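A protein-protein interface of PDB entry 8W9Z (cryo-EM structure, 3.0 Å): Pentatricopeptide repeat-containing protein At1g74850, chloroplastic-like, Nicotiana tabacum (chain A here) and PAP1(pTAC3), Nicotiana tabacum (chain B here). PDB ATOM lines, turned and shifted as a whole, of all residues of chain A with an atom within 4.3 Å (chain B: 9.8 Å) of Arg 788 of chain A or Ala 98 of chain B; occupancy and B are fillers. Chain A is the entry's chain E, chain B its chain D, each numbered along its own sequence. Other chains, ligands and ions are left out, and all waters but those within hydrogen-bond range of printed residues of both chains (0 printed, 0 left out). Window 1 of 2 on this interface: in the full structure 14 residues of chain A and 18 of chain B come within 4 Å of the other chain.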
ATOM      1  N   SER A 744     -25.895  -3.207 -16.265  1.00  0.00           N
ATOM      2  CA  SER A 744     -24.445  -3.305 -16.212  1.00  0.00           C
ATOM      3  C   SER A 744     -23.816  -2.663 -17.443  1.00  0.00           C
ATOM      4  O   SER A 744     -24.486  -2.377 -18.437  1.00  0.00           O
ATOM      5  CB  SER A 744     -24.000  -4.767 -16.104  1.00  0.00           C
ATOM      6  OG  SER A 744     -22.587  -4.869 -16.049  1.00  0.00           O
ATOM      7  N   VAL A 745     -22.509  -2.433 -17.355  1.00  0.00           N
ATOM      8  CA  VAL A 745     -21.712  -1.897 -18.456  1.00  0.00           C
ATOM      9  C   VAL A 745     -20.467  -2.770 -18.552  1.00  0.00           C
ATOM     10  O   VAL A 745     -19.506  -2.580 -17.798  1.00  0.00           O
ATOM     11  CB  VAL A 745     -21.339  -0.424 -18.255  1.00  0.00           C
ATOM     12  CG1 VAL A 745     -20.482   0.069 -19.412  1.00  0.00           C
ATOM     13  CG2 VAL A 745     -22.591   0.432 -18.116  1.00  0.00           C
ATOM     14  N   VAL A 746     -20.477  -3.727 -19.477  1.00  0.00           N
ATOM     15  CA  VAL A 746     -19.377  -4.678 -19.626  1.00  0.00           C
ATOM     16  C   VAL A 746     -18.222  -3.940 -20.296  1.00  0.00           C
ATOM     17  O   VAL A 746     -18.221  -3.736 -21.510  1.00  0.00           O
ATOM     18  CB  VAL A 746     -19.794  -5.916 -20.422  1.00  0.00           C
ATOM     19  CG1 VAL A 746     -18.669  -6.940 -20.439  1.00  0.00           C
ATOM     20  CG2 VAL A 746     -21.064  -6.517 -19.840  1.00  0.00           C
ATOM     21  N   VAL A 747     -17.232  -3.541 -19.504  1.00  0.00           N
ATOM     22  CA  VAL A 747     -16.079  -2.798 -20.001  1.00  0.00           C
ATOM     23  C   VAL A 747     -14.848  -3.687 -20.126  1.00  0.00           C
ATOM     24  O   VAL A 747     -14.130  -3.628 -21.125  1.00  0.00           O
ATOM     25  CB  VAL A 747     -15.805  -1.572 -19.098  1.00  0.00           C
ATOM     26  CG1 VAL A 747     -15.811  -1.970 -17.628  1.00  0.00           C
ATOM     27  CG2 VAL A 747     -14.489  -0.910 -19.476  1.00  0.00           C
ATOM     28  N   VAL A 748     -14.589  -4.526 -19.126  1.00  0.00           N
ATOM     29  CA  VAL A 748     -13.422  -5.402 -19.118  1.00  0.00           C
ATOM     30  C   VAL A 748     -13.853  -6.782 -18.640  1.00  0.00           C
ATOM     31  O   VAL A 748     -14.539  -6.908 -17.620  1.00  0.00           O
ATOM     32  CB  VAL A 748     -12.288  -4.841 -18.236  1.00  0.00           C
ATOM     33  CG1 VAL A 748     -12.827  -4.377 -16.891  1.00  0.00           C
ATOM     34  CG2 VAL A 748     -11.189  -5.876 -18.052  1.00  0.00           C
ATOM     35  N   GLU A 753     -10.824 -10.094 -14.256  1.00  0.00           N
ATOM     36  CA  GLU A 753     -11.979  -9.353 -13.735  1.00  0.00           C
ATOM     37  C   GLU A 753     -12.028  -9.196 -12.256  1.00  0.00           C
ATOM     38  O   GLU A 753     -12.425  -8.154 -11.763  1.00  0.00           O
ATOM     39  CB  GLU A 753     -13.215 -10.107 -14.109  1.00  0.00           C
ATOM     40  CG  GLU A 753     -13.940  -9.591 -15.333  1.00  0.00           C
ATOM     41  CD  GLU A 753     -15.080 -10.505 -15.733  1.00  0.00           C
ATOM     42  OE1 GLU A 753     -15.890 -10.114 -16.595  1.00  0.00           O
ATOM     43  OE2 GLU A 753     -15.168 -11.619 -15.176  1.00  0.00           O
ATOM     44  N   PHE A 781     -18.850   0.671  -9.395  1.00  0.00           N
ATOM     45  CA  PHE A 781     -18.286  -0.655  -9.586  1.00  0.00           C
ATOM     46  C   PHE A 781     -18.956  -1.655  -8.645  1.00  0.00           C
ATOM     47  O   PHE A 781     -19.300  -1.307  -7.511  1.00  0.00           O
ATOM     48  CB  PHE A 781     -16.779  -0.641  -9.334  1.00  0.00           C
ATOM     49  CG  PHE A 781     -15.985   0.035 -10.414  1.00  0.00           C
ATOM     50  CD1 PHE A 781     -15.774   1.404 -10.385  1.00  0.00           C
ATOM     51  CD2 PHE A 781     -15.439  -0.699 -11.454  1.00  0.00           C
ATOM     52  CE1 PHE A 781     -15.039   2.028 -11.376  1.00  0.00           C
ATOM     53  CE2 PHE A 781     -14.703  -0.082 -12.448  1.00  0.00           C
ATOM     54  CZ  PHE A 781     -14.503   1.283 -12.409  1.00  0.00           C
ATOM     55  N   PRO A 782     -19.154  -2.894  -9.081  1.00  0.00           N
ATOM     56  CA  PRO A 782     -19.729  -3.908  -8.194  1.00  0.00           C
ATOM     57  C   PRO A 782     -18.710  -4.426  -7.194  1.00  0.00           C
ATOM     58  O   PRO A 782     -17.497  -4.372  -7.412  1.00  0.00           O
ATOM     59  CB  PRO A 782     -20.160  -5.023  -9.159  1.00  0.00           C
ATOM     60  CG  PRO A 782     -20.053  -4.435 -10.541  1.00  0.00           C
ATOM     61  CD  PRO A 782     -18.992  -3.393 -10.453  1.00  0.00           C
ATOM     62  N   ASN A 785     -17.743  -8.350  -8.536  1.00  0.00           N
ATOM     63  CA  ASN A 785     -16.832  -8.388  -9.675  1.00  0.00           C
ATOM     64  C   ASN A 785     -16.452  -6.959 -10.027  1.00  0.00           C
ATOM     65  O   ASN A 785     -17.313  -6.165 -10.413  1.00  0.00           O
ATOM     66  CB  ASN A 785     -17.472  -9.090 -10.877  1.00  0.00           C
ATOM     67  CG  ASN A 785     -16.467  -9.429 -11.964  1.00  0.00           C
ATOM     68  OD1 ASN A 785     -15.458  -8.744 -12.134  1.00  0.00           O
ATOM     69  ND2 ASN A 785     -16.738 -10.496 -12.707  1.00  0.00           N
ATOM     70  N   LYS A 786     -15.167  -6.639  -9.899  1.00  0.00           N
ATOM     71  CA  LYS A 786     -14.671  -5.292 -10.180  1.00  0.00           C
ATOM     72  C   LYS A 786     -14.202  -5.188 -11.633  1.00  0.00           C
ATOM     73  O   LYS A 786     -13.049  -4.882 -11.930  1.00  0.00           O
ATOM     74  CB  LYS A 786     -13.554  -4.930  -9.209  1.00  0.00           C
ATOM     75  CG  LYS A 786     -13.950  -5.027  -7.745  1.00  0.00           C
ATOM     76  CD  LYS A 786     -12.751  -4.813  -6.835  1.00  0.00           C
ATOM     77  CE  LYS A 786     -11.679  -5.861  -7.085  1.00  0.00           C
ATOM     78  NZ  LYS A 786     -10.497  -5.673  -6.200  1.00  0.00           N
ATOM     79  N   GLY A 787     -15.132  -5.451 -12.547  1.00  0.00           N
ATOM     80  CA  GLY A 787     -14.810  -5.424 -13.960  1.00  0.00           C
ATOM     81  C   GLY A 787     -15.901  -4.835 -14.831  1.00  0.00           C
ATOM     82  O   GLY A 787     -15.917  -5.055 -16.046  1.00  0.00           O
ATOM     83  N   ARG A 788     -16.815  -4.082 -14.228  1.00  0.00           N
ATOM     84  CA  ARG A 788     -17.917  -3.477 -14.964  1.00  0.00           C
ATOM     85  C   ARG A 788     -18.492  -2.339 -14.130  1.00  0.00           C
ATOM     86  O   ARG A 788     -17.971  -1.998 -13.066  1.00  0.00           O
ATOM     87  CB  ARG A 788     -18.983  -4.519 -15.314  1.00  0.00           C
ATOM     88  CG  ARG A 788     -19.271  -5.503 -14.198  1.00  0.00           C
ATOM     89  CD  ARG A 788     -20.062  -6.689 -14.714  1.00  0.00           C
ATOM     90  NE  ARG A 788     -19.568  -7.157 -16.007  1.00  0.00           N
ATOM     91  CZ  ARG A 788     -18.480  -7.904 -16.172  1.00  0.00           C
ATOM     92  NH1 ARG A 788     -17.754  -8.269 -15.125  1.00  0.00           N
ATOM     93  NH2 ARG A 788     -18.113  -8.280 -17.389  1.00  0.00           N
ATOM     94  N   ILE A 789     -19.569  -1.745 -14.636  1.00  0.00           N
ATOM     95  CA  ILE A 789     -20.268  -0.654 -13.965  1.00  0.00           C
ATOM     96  C   ILE A 789     -21.741  -1.034 -13.905  1.00  0.00           C
ATOM     97  O   ILE A 789     -22.393  -1.166 -14.948  1.00  0.00           O
ATOM     98  CB  ILE A 789     -20.082   0.689 -14.683  1.00  0.00           C
ATOM     99  CG1 ILE A 789     -18.598   0.981 -14.912  1.00  0.00           C
ATOM    100  CG2 ILE A 789     -20.708   1.805 -13.871  1.00  0.00           C
ATOM    101  CD1 ILE A 789     -17.823   1.229 -13.640  1.00  0.00           C
ATOM    102  N   VAL A 790     -22.279  -1.155 -12.690  1.00  0.00           N
ATOM    103  CA  VAL A 790     -23.689  -1.523 -12.519  1.00  0.00           C
ATOM    104  C   VAL A 790     -24.546  -0.478 -11.822  1.00  0.00           C
ATOM    105  O   VAL A 790     -24.034   0.365 -11.087  1.00  0.00           O
ATOM    106  CB  VAL A 790     -23.844  -2.849 -11.748  1.00  0.00           C
ATOM    107  CG1 VAL A 790     -23.175  -3.991 -12.491  1.00  0.00           C
ATOM    108  CG2 VAL A 790     -23.299  -2.721 -10.334  1.00  0.00           C
ATOM    109  N   PHE B  73     -31.595 -14.770 -10.605  1.00  0.00           N
ATOM    110  CA  PHE B  73     -30.820 -15.337 -11.703  1.00  0.00           C
ATOM    111  C   PHE B  73     -31.078 -16.831 -11.849  1.00  0.00           C
ATOM    112  O   PHE B  73     -31.140 -17.348 -12.971  1.00  0.00           O
ATOM    113  CB  PHE B  73     -29.330 -15.069 -11.491  1.00  0.00           C
ATOM    114  CG  PHE B  73     -28.903 -13.678 -11.865  1.00  0.00           C
ATOM    115  CD1 PHE B  73     -29.728 -12.866 -12.626  1.00  0.00           C
ATOM    116  CD2 PHE B  73     -27.672 -13.185 -11.463  1.00  0.00           C
ATOM    117  CE1 PHE B  73     -29.335 -11.586 -12.973  1.00  0.00           C
ATOM    118  CE2 PHE B  73     -27.275 -11.908 -11.807  1.00  0.00           C
ATOM    119  CZ  PHE B  73     -28.108 -11.108 -12.562  1.00  0.00           C
ATOM    120  N   SER B  90     -29.456 -21.234 -22.000  1.00  0.00           N
ATOM    121  CA  SER B  90     -28.210 -20.732 -22.572  1.00  0.00           C
ATOM    122  C   SER B  90     -28.161 -19.209 -22.543  1.00  0.00           C
ATOM    123  O   SER B  90     -27.136 -18.620 -22.170  1.00  0.00           O
ATOM    124  CB  SER B  90     -28.043 -21.247 -24.001  1.00  0.00           C
ATOM    125  OG  SER B  90     -29.071 -20.755 -24.841  1.00  0.00           O
ATOM    126  N   GLN B  91     -29.259 -18.552 -22.925  1.00  0.00           N
ATOM    127  CA  GLN B  91     -29.262 -17.093 -22.908  1.00  0.00           C
ATOM    128  C   GLN B  91     -29.224 -16.552 -21.484  1.00  0.00           C
ATOM    129  O   GLN B  91     -28.617 -15.504 -21.241  1.00  0.00           O
ATOM    130  CB  GLN B  91     -30.472 -16.549 -23.678  1.00  0.00           C
ATOM    131  CG  GLN B  91     -31.829 -16.785 -23.037  1.00  0.00           C
ATOM    132  CD  GLN B  91     -32.253 -15.650 -22.124  1.00  0.00           C
ATOM    133  OE1 GLN B  91     -31.576 -14.626 -22.030  1.00  0.00           O
ATOM    134  NE2 GLN B  91     -33.382 -15.827 -21.447  1.00  0.00           N
ATOM    135  N   VAL B  92     -29.830 -17.258 -20.525  1.00  0.00           N
ATOM    136  CA  VAL B  92     -29.740 -16.829 -19.132  1.00  0.00           C
ATOM    137  C   VAL B  92     -28.310 -16.966 -18.622  1.00  0.00           C
ATOM    138  O   VAL B  92     -27.816 -16.107 -17.883  1.00  0.00           O
ATOM    139  CB  VAL B  92     -30.737 -17.615 -18.262  1.00  0.00           C
ATOM    140  CG1 VAL B  92     -30.457 -17.385 -16.786  1.00  0.00           C
ATOM    141  CG2 VAL B  92     -32.162 -17.202 -18.591  1.00  0.00           C
ATOM    142  N   ILE B  93     -27.618 -18.040 -19.014  1.00  0.00           N
ATOM    143  CA  ILE B  93     -26.218 -18.204 -18.629  1.00  0.00           C
ATOM    144  C   ILE B  93     -25.370 -17.087 -19.221  1.00  0.00           C
ATOM    145  O   ILE B  93     -24.502 -16.518 -18.546  1.00  0.00           O
ATOM    146  CB  ILE B  93     -25.704 -19.592 -19.053  1.00  0.00           C
ATOM    147  CG1 ILE B  93     -26.340 -20.685 -18.194  1.00  0.00           C
ATOM    148  CG2 ILE B  93     -24.186 -19.656 -18.963  1.00  0.00           C
ATOM    149  CD1 ILE B  93     -25.846 -22.077 -18.515  1.00  0.00           C
ATOM    150  N   TYR B  94     -25.607 -16.752 -20.492  1.00  0.00           N
ATOM    151  CA  TYR B  94     -24.865 -15.657 -21.111  1.00  0.00           C
ATOM    152  C   TYR B  94     -25.138 -14.333 -20.404  1.00  0.00           C
ATOM    153  O   TYR B  94     -24.216 -13.545 -20.163  1.00  0.00           O
ATOM    154  CB  TYR B  94     -25.212 -15.560 -22.596  1.00  0.00           C
ATOM    155  CG  TYR B  94     -24.505 -16.586 -23.451  1.00  0.00           C
ATOM    156  CD1 TYR B  94     -23.246 -17.057 -23.104  1.00  0.00           C
ATOM    157  CD2 TYR B  94     -25.096 -17.084 -24.604  1.00  0.00           C
ATOM    158  CE1 TYR B  94     -22.593 -17.994 -23.881  1.00  0.00           C
ATOM    159  CE2 TYR B  94     -24.452 -18.023 -25.389  1.00  0.00           C
ATOM    160  CZ  TYR B  94     -23.201 -18.474 -25.022  1.00  0.00           C
ATOM    161  OH  TYR B  94     -22.555 -19.408 -25.800  1.00  0.00           O
ATOM    162  N   ASP B  95     -26.400 -14.081 -20.047  1.00  0.00           N
ATOM    163  CA  ASP B  95     -26.738 -12.841 -19.358  1.00  0.00           C
ATOM    164  C   ASP B  95     -26.080 -12.772 -17.986  1.00  0.00           C
ATOM    165  O   ASP B  95     -25.590 -11.713 -17.578  1.00  0.00           O
ATOM    166  CB  ASP B  95     -28.255 -12.707 -19.232  1.00  0.00           C
ATOM    167  CG  ASP B  95     -28.941 -12.552 -20.575  1.00  0.00           C
ATOM    168  OD1 ASP B  95     -28.240 -12.591 -21.609  1.00  0.00           O
ATOM    169  OD2 ASP B  95     -30.179 -12.393 -20.598  1.00  0.00           O
ATOM    170  N   MET B  96     -26.056 -13.889 -17.258  1.00  0.00           N
ATOM    171  CA  MET B  96     -25.496 -13.870 -15.912  1.00  0.00           C
ATOM    172  C   MET B  96     -23.973 -13.817 -15.925  1.00  0.00           C
ATOM    173  O   MET B  96     -23.374 -13.267 -14.994  1.00  0.00           O
ATOM    174  CB  MET B  96     -25.980 -15.081 -15.110  1.00  0.00           C
ATOM    175  CG  MET B  96     -25.376 -16.404 -15.533  1.00  0.00           C
ATOM    176  SD  MET B  96     -25.886 -17.778 -14.487  1.00  0.00           S
ATOM    177  CE  MET B  96     -24.939 -19.108 -15.218  1.00  0.00           C
ATOM    178  N   ILE B  97     -23.327 -14.373 -16.953  1.00  0.00           N
ATOM    179  CA  ILE B  97     -21.878 -14.219 -17.048  1.00  0.00           C
ATOM    180  C   ILE B  97     -21.503 -12.848 -17.585  1.00  0.00           C
ATOM    181  O   ILE B  97     -20.380 -12.385 -17.350  1.00  0.00           O
ATOM    182  CB  ILE B  97     -21.234 -15.316 -17.915  1.00  0.00           C
ATOM    183  CG1 ILE B  97     -21.670 -15.189 -19.375  1.00  0.00           C
ATOM    184  CG2 ILE B  97     -21.559 -16.697 -17.364  1.00  0.00           C
ATOM    185  CD1 ILE B  97     -21.043 -16.216 -20.291  1.00  0.00           C
ATOM    186  N   ALA B  98     -22.412 -12.180 -18.299  1.00  0.00           N
ATOM    187  CA  ALA B  98     -22.170 -10.797 -18.689  1.00  0.00           C
ATOM    188  C   ALA B  98     -22.341  -9.835 -17.521  1.00  0.00           C
ATOM    189  O   ALA B  98     -21.783  -8.734 -17.554  1.00  0.00           O
ATOM    190  CB  ALA B  98     -23.101 -10.400 -19.834  1.00  0.00           C
ATOM    191  N   ALA B  99     -23.091 -10.227 -16.492  1.00  0.00           N
ATOM    192  CA  ALA B  99     -23.330  -9.372 -15.336  1.00  0.00           C
ATOM    193  C   ALA B  99     -22.184  -9.388 -14.334  1.00  0.00           C
ATOM    194  O   ALA B  99     -22.261  -8.683 -13.321  1.00  0.00           O
ATOM    195  CB  ALA B  99     -24.628  -9.783 -14.637  1.00  0.00           C
ATOM    196  N   GLY B 100     -21.129 -10.167 -14.581  1.00  0.00           N
ATOM    197  CA  GLY B 100     -19.956 -10.194 -13.743  1.00  0.00           C
ATOM    198  C   GLY B 100     -19.825 -11.432 -12.874  1.00  0.00           C
ATOM    199  O   GLY B 100     -18.705 -11.790 -12.492  1.00  0.00           O
ATOM    200  N   LEU B 101     -20.934 -12.090 -12.555  1.00  0.00           N
ATOM    201  CA  LEU B 101     -20.900 -13.251 -11.673  1.00  0.00           C
ATOM    202  C   LEU B 101     -20.488 -14.489 -12.460  1.00  0.00           C
ATOM    203  O   LEU B 101     -21.082 -14.801 -13.498  1.00  0.00           O
ATOM    204  CB  LEU B 101     -22.260 -13.462 -11.011  1.00  0.00           C
ATOM    205  CG  LEU B 101     -22.722 -12.362 -10.054  1.00  0.00           C
ATOM    206  CD1 LEU B 101     -23.620 -11.358 -10.763  1.00  0.00           C
ATOM    207  CD2 LEU B 101     -23.417 -12.964  -8.844  1.00  0.00           C
ATOM    208  N   SER B 102     -19.472 -15.191 -11.965  1.00  0.00           N
ATOM    209  CA  SER B 102     -19.038 -16.421 -12.605  1.00  0.00           C
ATOM    210  C   SER B 102     -20.099 -17.505 -12.426  1.00  0.00           C
ATOM    211  O   SER B 102     -20.742 -17.578 -11.373  1.00  0.00           O
ATOM    212  CB  SER B 102     -17.706 -16.888 -12.019  1.00  0.00           C
ATOM    213  OG  SER B 102     -17.299 -18.121 -12.585  1.00  0.00           O
ATOM    214  N   PRO B 103     -20.310 -18.354 -13.428  1.00  0.00           N
ATOM    215  CA  PRO B 103     -21.319 -19.408 -13.294  1.00  0.00           C
ATOM    216  C   PRO B 103     -20.882 -20.475 -12.304  1.00  0.00           C
ATOM    217  O   PRO B 103     -19.695 -20.775 -12.156  1.00  0.00           O
ATOM    218  CB  PRO B 103     -21.427 -19.977 -14.713  1.00  0.00           C
ATOM    219  CG  PRO B 103     -20.096 -19.693 -15.325  1.00  0.00           C
ATOM    220  CD  PRO B 103     -19.653 -18.379 -14.746  1.00  0.00           C
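O of Ala 98 of chain B sits at hydrogen-bond distance from NE of Arg 788 of chain A (3.1 Å). ND2 of Asn 785 of chain A lies close to O of Gly 100 of chain B (2.4 Å).
OD1 of Asn 785 of chain A lies close to O of Glu 753 of chain A, 3.1 Å away. The side-chain carboxylate (OE1) of Glu 753 of chain A is in salt-bridge range of the guanidinium group (NH2) of Arg 788 of chain A (3.0 Å). The side-chain amide oxygen of Asn 785 of chain A sits close to the backbone NH of Gly 787 of chain A, at 3.3 Å. NH1 of Arg 788 of chain A sits close to ND2 of Asn 785 of chain A.
Val 746 of chain A touches Ala 98 of chain B (CG2 to O, 3.3 Å). Ala 99 of chain B touches Arg 788 of chain A (O to CD, 3.3 Å). NH1 of Arg 788 of chain A touches CA of Gly 100 of chain B, at 3.2 Å.
Arg 788 of chain A touches just these residues of chain B: Ala 98 (3.1 Å), Ala 99 (3.3 Å) and Gly 100 (3.2 Å). Gly 787 of chain A touches none of the printed residues of chain B. No residue of chain B comes within 4 Å of Ile 789 of chain A. Printed residues of chain A within 4 Å of Gly 100 of chain B: Asn 785 and Arg 788. Of the printed residues of chain A, Ala 99 of chain B touches Arg 788. Val 748 of chain A touches none of the printed residues of chain B. The nearest residue of chain B that does not touch Arg 788 of chain A is Ile 97 of chain B (4.7 Å).
Of the 15 printed residues of chain B, 3 touch a printed residue of chain A. Of the 14 printed residues of chain A, 3 touch a printed residue of chain B. Hydrophobic or aromatic side chains of chain A within 4 Å of the printed part of chain B: Val 746. Among the printed residues, no Asp or Glu carboxylate lies within 4 Å of a Lys or Arg side-chain nitrogen of the other chain.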
